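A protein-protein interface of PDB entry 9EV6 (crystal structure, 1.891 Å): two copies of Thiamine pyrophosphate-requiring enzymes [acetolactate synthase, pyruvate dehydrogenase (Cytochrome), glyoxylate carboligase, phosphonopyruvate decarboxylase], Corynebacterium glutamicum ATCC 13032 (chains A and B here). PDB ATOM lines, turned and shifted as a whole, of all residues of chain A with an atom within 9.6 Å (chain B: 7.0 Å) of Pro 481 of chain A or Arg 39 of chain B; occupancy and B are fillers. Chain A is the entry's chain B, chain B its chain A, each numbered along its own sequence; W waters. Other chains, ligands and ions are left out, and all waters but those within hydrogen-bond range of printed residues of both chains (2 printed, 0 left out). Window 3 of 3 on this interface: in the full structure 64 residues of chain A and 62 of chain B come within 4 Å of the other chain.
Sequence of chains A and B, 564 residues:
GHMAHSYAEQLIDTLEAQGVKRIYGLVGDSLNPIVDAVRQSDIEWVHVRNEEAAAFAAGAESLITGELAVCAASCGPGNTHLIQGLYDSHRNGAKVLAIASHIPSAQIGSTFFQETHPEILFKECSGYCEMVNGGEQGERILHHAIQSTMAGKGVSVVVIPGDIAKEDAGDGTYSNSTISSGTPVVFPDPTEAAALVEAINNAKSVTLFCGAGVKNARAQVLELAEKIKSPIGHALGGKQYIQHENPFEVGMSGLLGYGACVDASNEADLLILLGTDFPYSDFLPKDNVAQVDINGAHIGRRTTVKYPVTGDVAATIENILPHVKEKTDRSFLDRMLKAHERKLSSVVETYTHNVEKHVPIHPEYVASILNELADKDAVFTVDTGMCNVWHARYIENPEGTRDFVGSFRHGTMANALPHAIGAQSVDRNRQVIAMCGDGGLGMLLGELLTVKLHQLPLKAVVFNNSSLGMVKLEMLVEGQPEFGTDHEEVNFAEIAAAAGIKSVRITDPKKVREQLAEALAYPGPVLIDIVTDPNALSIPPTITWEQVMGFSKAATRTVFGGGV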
ATOM      1  N   VAL A 471      19.067 -20.692  -1.538  1.00  0.00           N
ATOM      2  CA  VAL A 471      20.201 -19.775  -1.396  1.00  0.00           C
ATOM      3  C   VAL A 471      21.354 -20.460  -0.675  1.00  0.00           C
ATOM      4  O   VAL A 471      22.507 -20.324  -1.077  1.00  0.00           O
ATOM      5  CB  VAL A 471      19.779 -18.488  -0.666  1.00  0.00           C
ATOM      6  CG1 VAL A 471      20.951 -17.511  -0.562  1.00  0.00           C
ATOM      7  CG2 VAL A 471      18.580 -17.848  -1.369  1.00  0.00           C
ATOM      8  N   LYS A 472      21.036 -21.292   0.340  1.00  0.00           N
ATOM      9  CA  LYS A 472      22.008 -22.097   1.076  1.00  0.00           C
ATOM     10  C   LYS A 472      22.808 -22.972   0.086  1.00  0.00           C
ATOM     11  O   LYS A 472      24.038 -22.997   0.131  1.00  0.00           O
ATOM     12  CB  LYS A 472      21.220 -22.978   2.061  1.00  0.00           C
ATOM     13  CG  LYS A 472      21.785 -23.157   3.423  1.00  0.00           C
ATOM     14  CD  LYS A 472      20.832 -24.075   4.205  1.00  0.00           C
ATOM     15  CE  LYS A 472      21.567 -24.936   5.175  1.00  0.00           C
ATOM     16  NZ  LYS A 472      22.055 -24.175   6.348  1.00  0.00           N
ATOM     17  N   GLU A 474      23.014 -22.433  -3.349  1.00  0.00           N
ATOM     18  CA  GLU A 474      23.775 -21.531  -4.230  1.00  0.00           C
ATOM     19  C   GLU A 474      25.115 -21.138  -3.583  1.00  0.00           C
ATOM     20  O   GLU A 474      26.139 -21.136  -4.253  1.00  0.00           O
ATOM     21  CB  GLU A 474      22.994 -20.234  -4.524  1.00  0.00           C
ATOM     22  CG  GLU A 474      21.705 -20.352  -5.314  1.00  0.00           C
ATOM     23  CD  GLU A 474      20.903 -19.055  -5.355  1.00  0.00           C
ATOM     24  OE1 GLU A 474      20.018 -18.927  -6.231  1.00  0.00           O
ATOM     25  OE2 GLU A 474      21.153 -18.165  -4.512  1.00  0.00           O
ATOM     26  N   MET A 475      25.096 -20.793  -2.291  1.00  0.00           N
ATOM     27  CA  MET A 475      26.302 -20.379  -1.588  1.00  0.00           C
ATOM     28  C   MET A 475      27.298 -21.549  -1.443  1.00  0.00           C
ATOM     29  O   MET A 475      28.494 -21.333  -1.560  1.00  0.00           O
ATOM     30  CB  MET A 475      25.942 -19.796  -0.215  1.00  0.00           C
ATOM     31  CG  MET A 475      25.218 -18.481  -0.329  1.00  0.00           C
ATOM     32  SD  MET A 475      24.787 -17.744   1.272  1.00  0.00           S
ATOM     33  CE  MET A 475      24.196 -16.128   0.711  1.00  0.00           C
ATOM     34  N   LEU A 476      26.806 -22.775  -1.233  1.00  0.00           N
ATOM     35  CA  LEU A 476      27.672 -23.942  -1.150  1.00  0.00           C
ATOM     36  C   LEU A 476      28.361 -24.176  -2.504  1.00  0.00           C
ATOM     37  O   LEU A 476      29.575 -24.363  -2.545  1.00  0.00           O
ATOM     38  CB  LEU A 476      26.860 -25.170  -0.724  1.00  0.00           C
ATOM     39  CG  LEU A 476      27.652 -26.468  -0.517  1.00  0.00           C
ATOM     40  CD1 LEU A 476      28.534 -26.403   0.736  1.00  0.00           C
ATOM     41  CD2 LEU A 476      26.712 -27.653  -0.399  1.00  0.00           C
ATOM     42  N   VAL A 477      27.603 -24.084  -3.610  1.00  0.00           N
ATOM     43  CA  VAL A 477      28.114 -24.275  -4.967  1.00  0.00           C
ATOM     44  C   VAL A 477      29.154 -23.201  -5.313  1.00  0.00           C
ATOM     45  O   VAL A 477      30.196 -23.527  -5.874  1.00  0.00           O
ATOM     46  CB  VAL A 477      26.942 -24.298  -5.991  1.00  0.00           C
ATOM     47  CG1 VAL A 477      27.426 -24.078  -7.421  1.00  0.00           C
ATOM     48  CG2 VAL A 477      26.156 -25.604  -5.890  1.00  0.00           C
ATOM     49  N   GLU A 478      28.890 -21.931  -4.962  1.00  0.00           N
ATOM     50  CA  GLU A 478      29.810 -20.823  -5.246  1.00  0.00           C
ATOM     51  C   GLU A 478      31.039 -20.768  -4.327  1.00  0.00           C
ATOM     52  O   GLU A 478      31.874 -19.895  -4.524  1.00  0.00           O
ATOM     53  CB  GLU A 478      29.084 -19.482  -5.115  1.00  0.00           C
ATOM     54  CG  GLU A 478      28.064 -19.178  -6.197  1.00  0.00           C
ATOM     55  CD  GLU A 478      27.273 -17.912  -5.903  1.00  0.00           C
ATOM     56  OE1 GLU A 478      26.436 -17.932  -4.969  1.00  0.00           O
ATOM     57  OE2 GLU A 478      27.512 -16.892  -6.590  1.00  0.00           O
ATOM     58  N   GLY A 479      31.112 -21.624  -3.307  1.00  0.00           N
ATOM     59  CA  GLY A 479      32.217 -21.597  -2.360  1.00  0.00           C
ATOM     60  C   GLY A 479      32.143 -20.435  -1.386  1.00  0.00           C
ATOM     61  O   GLY A 479      33.164 -19.965  -0.886  1.00  0.00           O
ATOM     62  N   GLN A 480      30.935 -19.975  -1.091  1.00  0.00           N
ATOM     63  CA  GLN A 480      30.711 -18.845  -0.202  1.00  0.00           C
ATOM     64  C   GLN A 480      30.279 -19.284   1.188  1.00  0.00           C
ATOM     65  O   GLN A 480      29.317 -20.038   1.314  1.00  0.00           O
ATOM     66  CB  GLN A 480      29.621 -17.959  -0.814  1.00  0.00           C
ATOM     67  CG  GLN A 480      29.218 -16.754   0.028  1.00  0.00           C
ATOM     68  CD  GLN A 480      28.208 -15.881  -0.686  1.00  0.00           C
ATOM     69  OE1 GLN A 480      28.056 -15.927  -1.910  1.00  0.00           O
ATOM     70  NE2 GLN A 480      27.496 -15.064   0.063  1.00  0.00           N
ATOM     71  N   PRO A 481      30.910 -18.760   2.264  1.00  0.00           N
ATOM     72  CA  PRO A 481      30.458 -19.118   3.616  1.00  0.00           C
ATOM     73  C   PRO A 481      29.013 -18.666   3.810  1.00  0.00           C
ATOM     74  O   PRO A 481      28.642 -17.561   3.386  1.00  0.00           O
ATOM     75  CB  PRO A 481      31.428 -18.361   4.533  1.00  0.00           C
ATOM     76  CG  PRO A 481      32.612 -18.064   3.676  1.00  0.00           C
ATOM     77  CD  PRO A 481      32.044 -17.823   2.307  1.00  0.00           C
ATOM     78  N   GLU A 482      28.180 -19.569   4.322  1.00  0.00           N
ATOM     79  CA  GLU A 482      26.761 -19.337   4.493  1.00  0.00           C
ATOM     80  C   GLU A 482      26.474 -18.129   5.366  1.00  0.00           C
ATOM     81  O   GLU A 482      27.099 -17.962   6.402  1.00  0.00           O
ATOM     82  CB  GLU A 482      26.110 -20.574   5.099  1.00  0.00           C
ATOM     83  CG  GLU A 482      24.600 -20.560   5.007  1.00  0.00           C
ATOM     84  CD  GLU A 482      23.989 -21.643   5.867  1.00  0.00           C
ATOM     85  OE1 GLU A 482      24.331 -22.827   5.640  1.00  0.00           O
ATOM     86  OE2 GLU A 482      23.199 -21.314   6.784  1.00  0.00           O
ATOM     87  N   PHE A 483      25.544 -17.279   4.932  1.00  0.00           N
ATOM     88  CA  PHE A 483      25.183 -16.092   5.687  1.00  0.00           C
ATOM     89  C   PHE A 483      23.812 -15.585   5.260  1.00  0.00           C
ATOM     90  O   PHE A 483      23.522 -15.504   4.072  1.00  0.00           O
ATOM     91  CB  PHE A 483      26.246 -14.991   5.474  1.00  0.00           C
ATOM     92  CG  PHE A 483      26.102 -13.793   6.382  1.00  0.00           C
ATOM     93  CD1 PHE A 483      26.595 -13.821   7.678  1.00  0.00           C
ATOM     94  CD2 PHE A 483      25.494 -12.633   5.934  1.00  0.00           C
ATOM     95  CE1 PHE A 483      26.474 -12.709   8.505  1.00  0.00           C
ATOM     96  CE2 PHE A 483      25.381 -11.521   6.761  1.00  0.00           C
ATOM     97  CZ  PHE A 483      25.869 -11.566   8.039  1.00  0.00           C
ATOM     98  N   GLY A 484      22.991 -15.225   6.226  1.00  0.00           N
ATOM     99  CA  GLY A 484      21.689 -14.630   5.966  1.00  0.00           C
ATOM    100  C   GLY A 484      20.609 -15.544   5.437  1.00  0.00           C
ATOM    101  O   GLY A 484      19.541 -15.071   5.057  1.00  0.00           O
ATOM    102  N   THR A 485      20.855 -16.857   5.424  1.00  0.00           N
ATOM    103  CA  THR A 485      19.883 -17.796   4.863  1.00  0.00           C
ATOM    104  C   THR A 485      19.066 -18.496   5.927  1.00  0.00           C
ATOM    105  O   THR A 485      17.896 -18.776   5.681  1.00  0.00           O
ATOM    106  CB  THR A 485      20.586 -18.833   3.981  1.00  0.00           C
ATOM    107  OG1 THR A 485      21.405 -19.662   4.798  1.00  0.00           O
ATOM    108  CG2 THR A 485      21.459 -18.184   2.917  1.00  0.00           C
ATOM    109  N   ILE B  12      30.332  -2.138  -0.304  1.00  0.00           N
ATOM    110  CA  ILE B  12      30.054  -2.248   1.122  1.00  0.00           C
ATOM    111  C   ILE B  12      31.045  -1.435   1.939  1.00  0.00           C
ATOM    112  O   ILE B  12      30.623  -0.740   2.880  1.00  0.00           O
ATOM    113  CB  ILE B  12      30.028  -3.741   1.535  1.00  0.00           C
ATOM    114  CG1 ILE B  12      28.821  -4.451   0.869  1.00  0.00           C
ATOM    115  CG2 ILE B  12      29.999  -3.912   3.029  1.00  0.00           C
ATOM    116  CD1 ILE B  12      27.491  -3.800   1.167  1.00  0.00           C
ATOM    117  N   ILE B  34      27.273  -9.578  -2.702  1.00  0.00           N
ATOM    118  CA  ILE B  34      27.132  -8.374  -1.900  1.00  0.00           C
ATOM    119  C   ILE B  34      26.921  -8.744  -0.420  1.00  0.00           C
ATOM    120  O   ILE B  34      27.569  -8.154   0.445  1.00  0.00           O
ATOM    121  CB  ILE B  34      26.023  -7.465  -2.439  1.00  0.00           C
ATOM    122  CG1 ILE B  34      26.433  -6.954  -3.844  1.00  0.00           C
ATOM    123  CG2 ILE B  34      25.719  -6.325  -1.463  1.00  0.00           C
ATOM    124  CD1 ILE B  34      25.498  -6.049  -4.490  1.00  0.00           C
ATOM    125  N   VAL B  35      26.089  -9.739  -0.127  1.00  0.00           N
ATOM    126  CA  VAL B  35      25.878 -10.182   1.260  1.00  0.00           C
ATOM    127  C   VAL B  35      27.170 -10.842   1.815  1.00  0.00           C
ATOM    128  O   VAL B  35      27.406 -10.778   3.024  1.00  0.00           O
ATOM    129  CB  VAL B  35      24.633 -11.095   1.358  1.00  0.00           C
ATOM    130  CG1 VAL B  35      24.609 -11.932   2.632  1.00  0.00           C
ATOM    131  CG2 VAL B  35      23.349 -10.285   1.212  1.00  0.00           C
ATOM    132  N   ASP B  36      28.027 -11.423   0.947  1.00  0.00           N
ATOM    133  CA  ASP B  36      29.317 -11.940   1.402  1.00  0.00           C
ATOM    134  C   ASP B  36      30.203 -10.779   1.858  1.00  0.00           C
ATOM    135  O   ASP B  36      30.964 -10.922   2.821  1.00  0.00           O
ATOM    136  CB  ASP B  36      30.037 -12.736   0.317  1.00  0.00           C
ATOM    137  CG  ASP B  36      31.288 -13.406   0.854  1.00  0.00           C
ATOM    138  OD1 ASP B  36      31.157 -14.326   1.683  1.00  0.00           O
ATOM    139  OD2 ASP B  36      32.394 -12.996   0.465  1.00  0.00           O
ATOM    140  N   ALA B  37      30.116  -9.632   1.175  1.00  0.00           N
ATOM    141  CA  ALA B  37      30.875  -8.460   1.552  1.00  0.00           C
ATOM    142  C   ALA B  37      30.284  -7.862   2.814  1.00  0.00           C
ATOM    143  O   ALA B  37      31.066  -7.444   3.667  1.00  0.00           O
ATOM    144  CB  ALA B  37      30.882  -7.448   0.427  1.00  0.00           C
ATOM    145  N   VAL B  38      28.924  -7.883   3.003  1.00  0.00           N
ATOM    146  CA  VAL B  38      28.371  -7.367   4.255  1.00  0.00           C
ATOM    147  C   VAL B  38      28.815  -8.293   5.414  1.00  0.00           C
ATOM    148  O   VAL B  38      29.207  -7.776   6.457  1.00  0.00           O
ATOM    149  CB  VAL B  38      26.868  -6.984   4.317  1.00  0.00           C
ATOM    150  CG1 VAL B  38      26.173  -6.852   2.971  1.00  0.00           C
ATOM    151  CG2 VAL B  38      26.060  -7.660   5.402  1.00  0.00           C
ATOM    152  N   ARG B  39      28.899  -9.624   5.183  1.00  0.00           N
ATOM    153  CA  ARG B  39      29.381 -10.577   6.190  1.00  0.00           C
ATOM    154  C   ARG B  39      30.785 -10.179   6.701  1.00  0.00           C
ATOM    155  O   ARG B  39      31.015 -10.208   7.898  1.00  0.00           O
ATOM    156  CB  ARG B  39      29.421 -12.011   5.632  1.00  0.00           C
ATOM    157  CG  ARG B  39      30.001 -13.029   6.633  1.00  0.00           C
ATOM    158  CD  ARG B  39      30.281 -14.396   6.049  1.00  0.00           C
ATOM    159  NE  ARG B  39      31.161 -14.340   4.882  1.00  0.00           N
ATOM    160  CZ  ARG B  39      32.486 -14.428   4.928  1.00  0.00           C
ATOM    161  NH1 ARG B  39      33.110 -14.541   6.091  1.00  0.00           N
ATOM    162  NH2 ARG B  39      33.197 -14.382   3.812  1.00  0.00           N
ATOM    163  N   GLN B  40      31.689  -9.785   5.798  1.00  0.00           N
ATOM    164  CA  GLN B  40      33.051  -9.408   6.172  1.00  0.00           C
ATOM    165  C   GLN B  40      33.174  -7.983   6.719  1.00  0.00           C
ATOM    166  O   GLN B  40      34.225  -7.629   7.228  1.00  0.00           O
ATOM    167  CB  GLN B  40      33.975  -9.527   4.959  1.00  0.00           C
ATOM    168  CG  GLN B  40      34.062 -10.920   4.404  1.00  0.00           C
ATOM    169  CD  GLN B  40      34.868 -10.879   3.133  1.00  0.00           C
ATOM    170  OE1 GLN B  40      34.323 -10.831   2.030  1.00  0.00           O
ATOM    171  NE2 GLN B  40      36.185 -10.858   3.243  1.00  0.00           N
ATOM    172  N   SER B  41      32.140  -7.168   6.598  1.00  0.00           N
ATOM    173  CA  SER B  41      32.153  -5.794   7.076  1.00  0.00           C
ATOM    174  C   SER B  41      31.548  -5.702   8.483  1.00  0.00           C
ATOM    175  O   SER B  41      31.102  -6.705   9.032  1.00  0.00           O
ATOM    176  CB  SER B  41      31.352  -4.938   6.098  1.00  0.00           C
ATOM    177  OG  SER B  41      29.957  -5.022   6.353  1.00  0.00           O
ATOM    178  N   ASP B  42      31.449  -4.494   9.018  1.00  0.00           N
ATOM    179  CA  ASP B  42      30.831  -4.266  10.308  1.00  0.00           C
ATOM    180  C   ASP B  42      29.387  -3.739  10.141  1.00  0.00           C
ATOM    181  O   ASP B  42      28.796  -3.271  11.117  1.00  0.00           O
ATOM    182  CB  ASP B  42      31.697  -3.298  11.108  1.00  0.00           C
ATOM    183  CG  ASP B  42      33.147  -3.711  10.978  1.00  0.00           C
ATOM    184  OD1 ASP B  42      33.461  -4.884  11.305  1.00  0.00           O
ATOM    185  OD2 ASP B  42      33.950  -2.906  10.442  1.00  0.00           O
ATOM    186  N   ILE B  43      28.799  -3.847   8.935  1.00  0.00           N
ATOM    187  CA  ILE B  43      27.416  -3.456   8.730  1.00  0.00           C
ATOM    188  C   ILE B  43      26.523  -4.633   9.131  1.00  0.00           C
ATOM    189  O   ILE B  43      26.819  -5.776   8.789  1.00  0.00           O
ATOM    190  CB  ILE B  43      27.183  -3.039   7.245  1.00  0.00           C
ATOM    191  CG1 ILE B  43      27.908  -1.736   6.927  1.00  0.00           C
ATOM    192  CG2 ILE B  43      25.695  -2.948   6.884  1.00  0.00           C
ATOM    193  CD1 ILE B  43      27.771  -1.309   5.403  1.00  0.00           C
ATOM    194  N   TRP B  45      23.284  -7.003   8.796  1.00  0.00           N
ATOM    195  CA  TRP B  45      22.331  -7.443   7.794  1.00  0.00           C
ATOM    196  C   TRP B  45      21.012  -7.688   8.501  1.00  0.00           C
ATOM    197  O   TRP B  45      20.961  -8.512   9.436  1.00  0.00           O
ATOM    198  CB  TRP B  45      22.822  -8.729   7.106  1.00  0.00           C
ATOM    199  CG  TRP B  45      21.866  -9.233   6.067  1.00  0.00           C
ATOM    200  CD1 TRP B  45      21.028 -10.308   6.165  1.00  0.00           C
ATOM    201  CD2 TRP B  45      21.608  -8.640   4.797  1.00  0.00           C
ATOM    202  NE1 TRP B  45      20.309 -10.453   5.002  1.00  0.00           N
ATOM    203  CE2 TRP B  45      20.626  -9.427   4.155  1.00  0.00           C
ATOM    204  CE3 TRP B  45      22.152  -7.554   4.113  1.00  0.00           C
ATOM    205  CZ2 TRP B  45      20.173  -9.143   2.859  1.00  0.00           C
ATOM    206  CZ3 TRP B  45      21.696  -7.265   2.842  1.00  0.00           C
ATOM    207  CH2 TRP B  45      20.714  -8.047   2.229  1.00  0.00           C
HETATM  208  O   HOH W   1      18.450 -12.624   4.221  1.00  0.00           O
HETATM  209  O   HOH W   2      28.834 -14.982   2.858  1.00  0.00           O
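Water W2 lies within hydrogen-bond range of the backbone carbonyl oxygen of Pro 481 of chain A, the side-chain carboxylate of Asp 36 of chain B, the side-chain amide nitrogen of Gln 480 of chain A and the guanidinium group of Arg 39 of chain B. Water W1 bridges O of Gly 484 of chain A (2.8 Å) and NE1 of Trp 45 of chain B (3.0 Å).
No position is printed for both chains. Of the 6 pairs that touch across the chains among the printed residues, none has its exchanged pair printed and touching as well.
Of the 14 printed residues of chain A, 3 touch a printed residue of chain B. Hydrophobic or aromatic side chains of chain A within 4 Å of the printed part of chain B: Pro 481 and Phe 483. Among the printed residues, 6 pairs touch across the chains. Among the printed residues, no Asp or Glu carboxylate lies within 4 Å of a Lys or Arg side-chain nitrogen of the other chain.
Pro 481 of chain A touches just these residues of chain B: Asp 36 and Arg 39. Of the printed residues of chain A, Val 35 of chain B touches Phe 483 (3.5 Å). Of the printed residues of chain A, Asp 36 of chain B touches Gln 480 (3.5 Å) and Pro 481 (3.7 Å). Ala 37 of chain B touches none of the printed residues of chain A. Arg 39 of chain B touches just these residues of chain A: Pro 481 and Phe 483. No residue of chain A comes within 4 Å of Gln 40 of chain B. No residue of chain A comes within 4 Å of Ser 41 of chain B. Of the printed residues of chain A, Trp 45 of chain B touches Phe 483.
Asp 36 of chain B touches Gln 480 of chain A. Asp 36 of chain B touches Pro 481 of chain A (OD1 to CD, 3.7 Å). NH2 of Arg 39 of chain B touches CG of Pro 481 of chain A, at 3.7 Å. Phe 483 of chain A touches Val 35 of chain B. Arg 39 of chain B touches Phe 483 of chain A. CB of Trp 45 of chain B touches CE2 of Phe 483 of chain A, at 3.8 Å.
The backbone carbonyl oxygen (O) of Met 475 of chain A is in hydrogen-bond range of the backbone NH (N) of Gln 480 of chain A (2.8 Å). The side-chain sulfur of Met 475 of chain A sits at hydrogen-bond distance from the backbone NH of Phe 483 of chain A, at 3.8 Å. OD2 of Asp 36 of chain B lies close to OE1 of Gln 40 of chain B (3.3 Å). OD1 of Asp 36 of chain B lies within salt-bridge range of NH2 of Arg 39 of chain B (2.9 Å).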
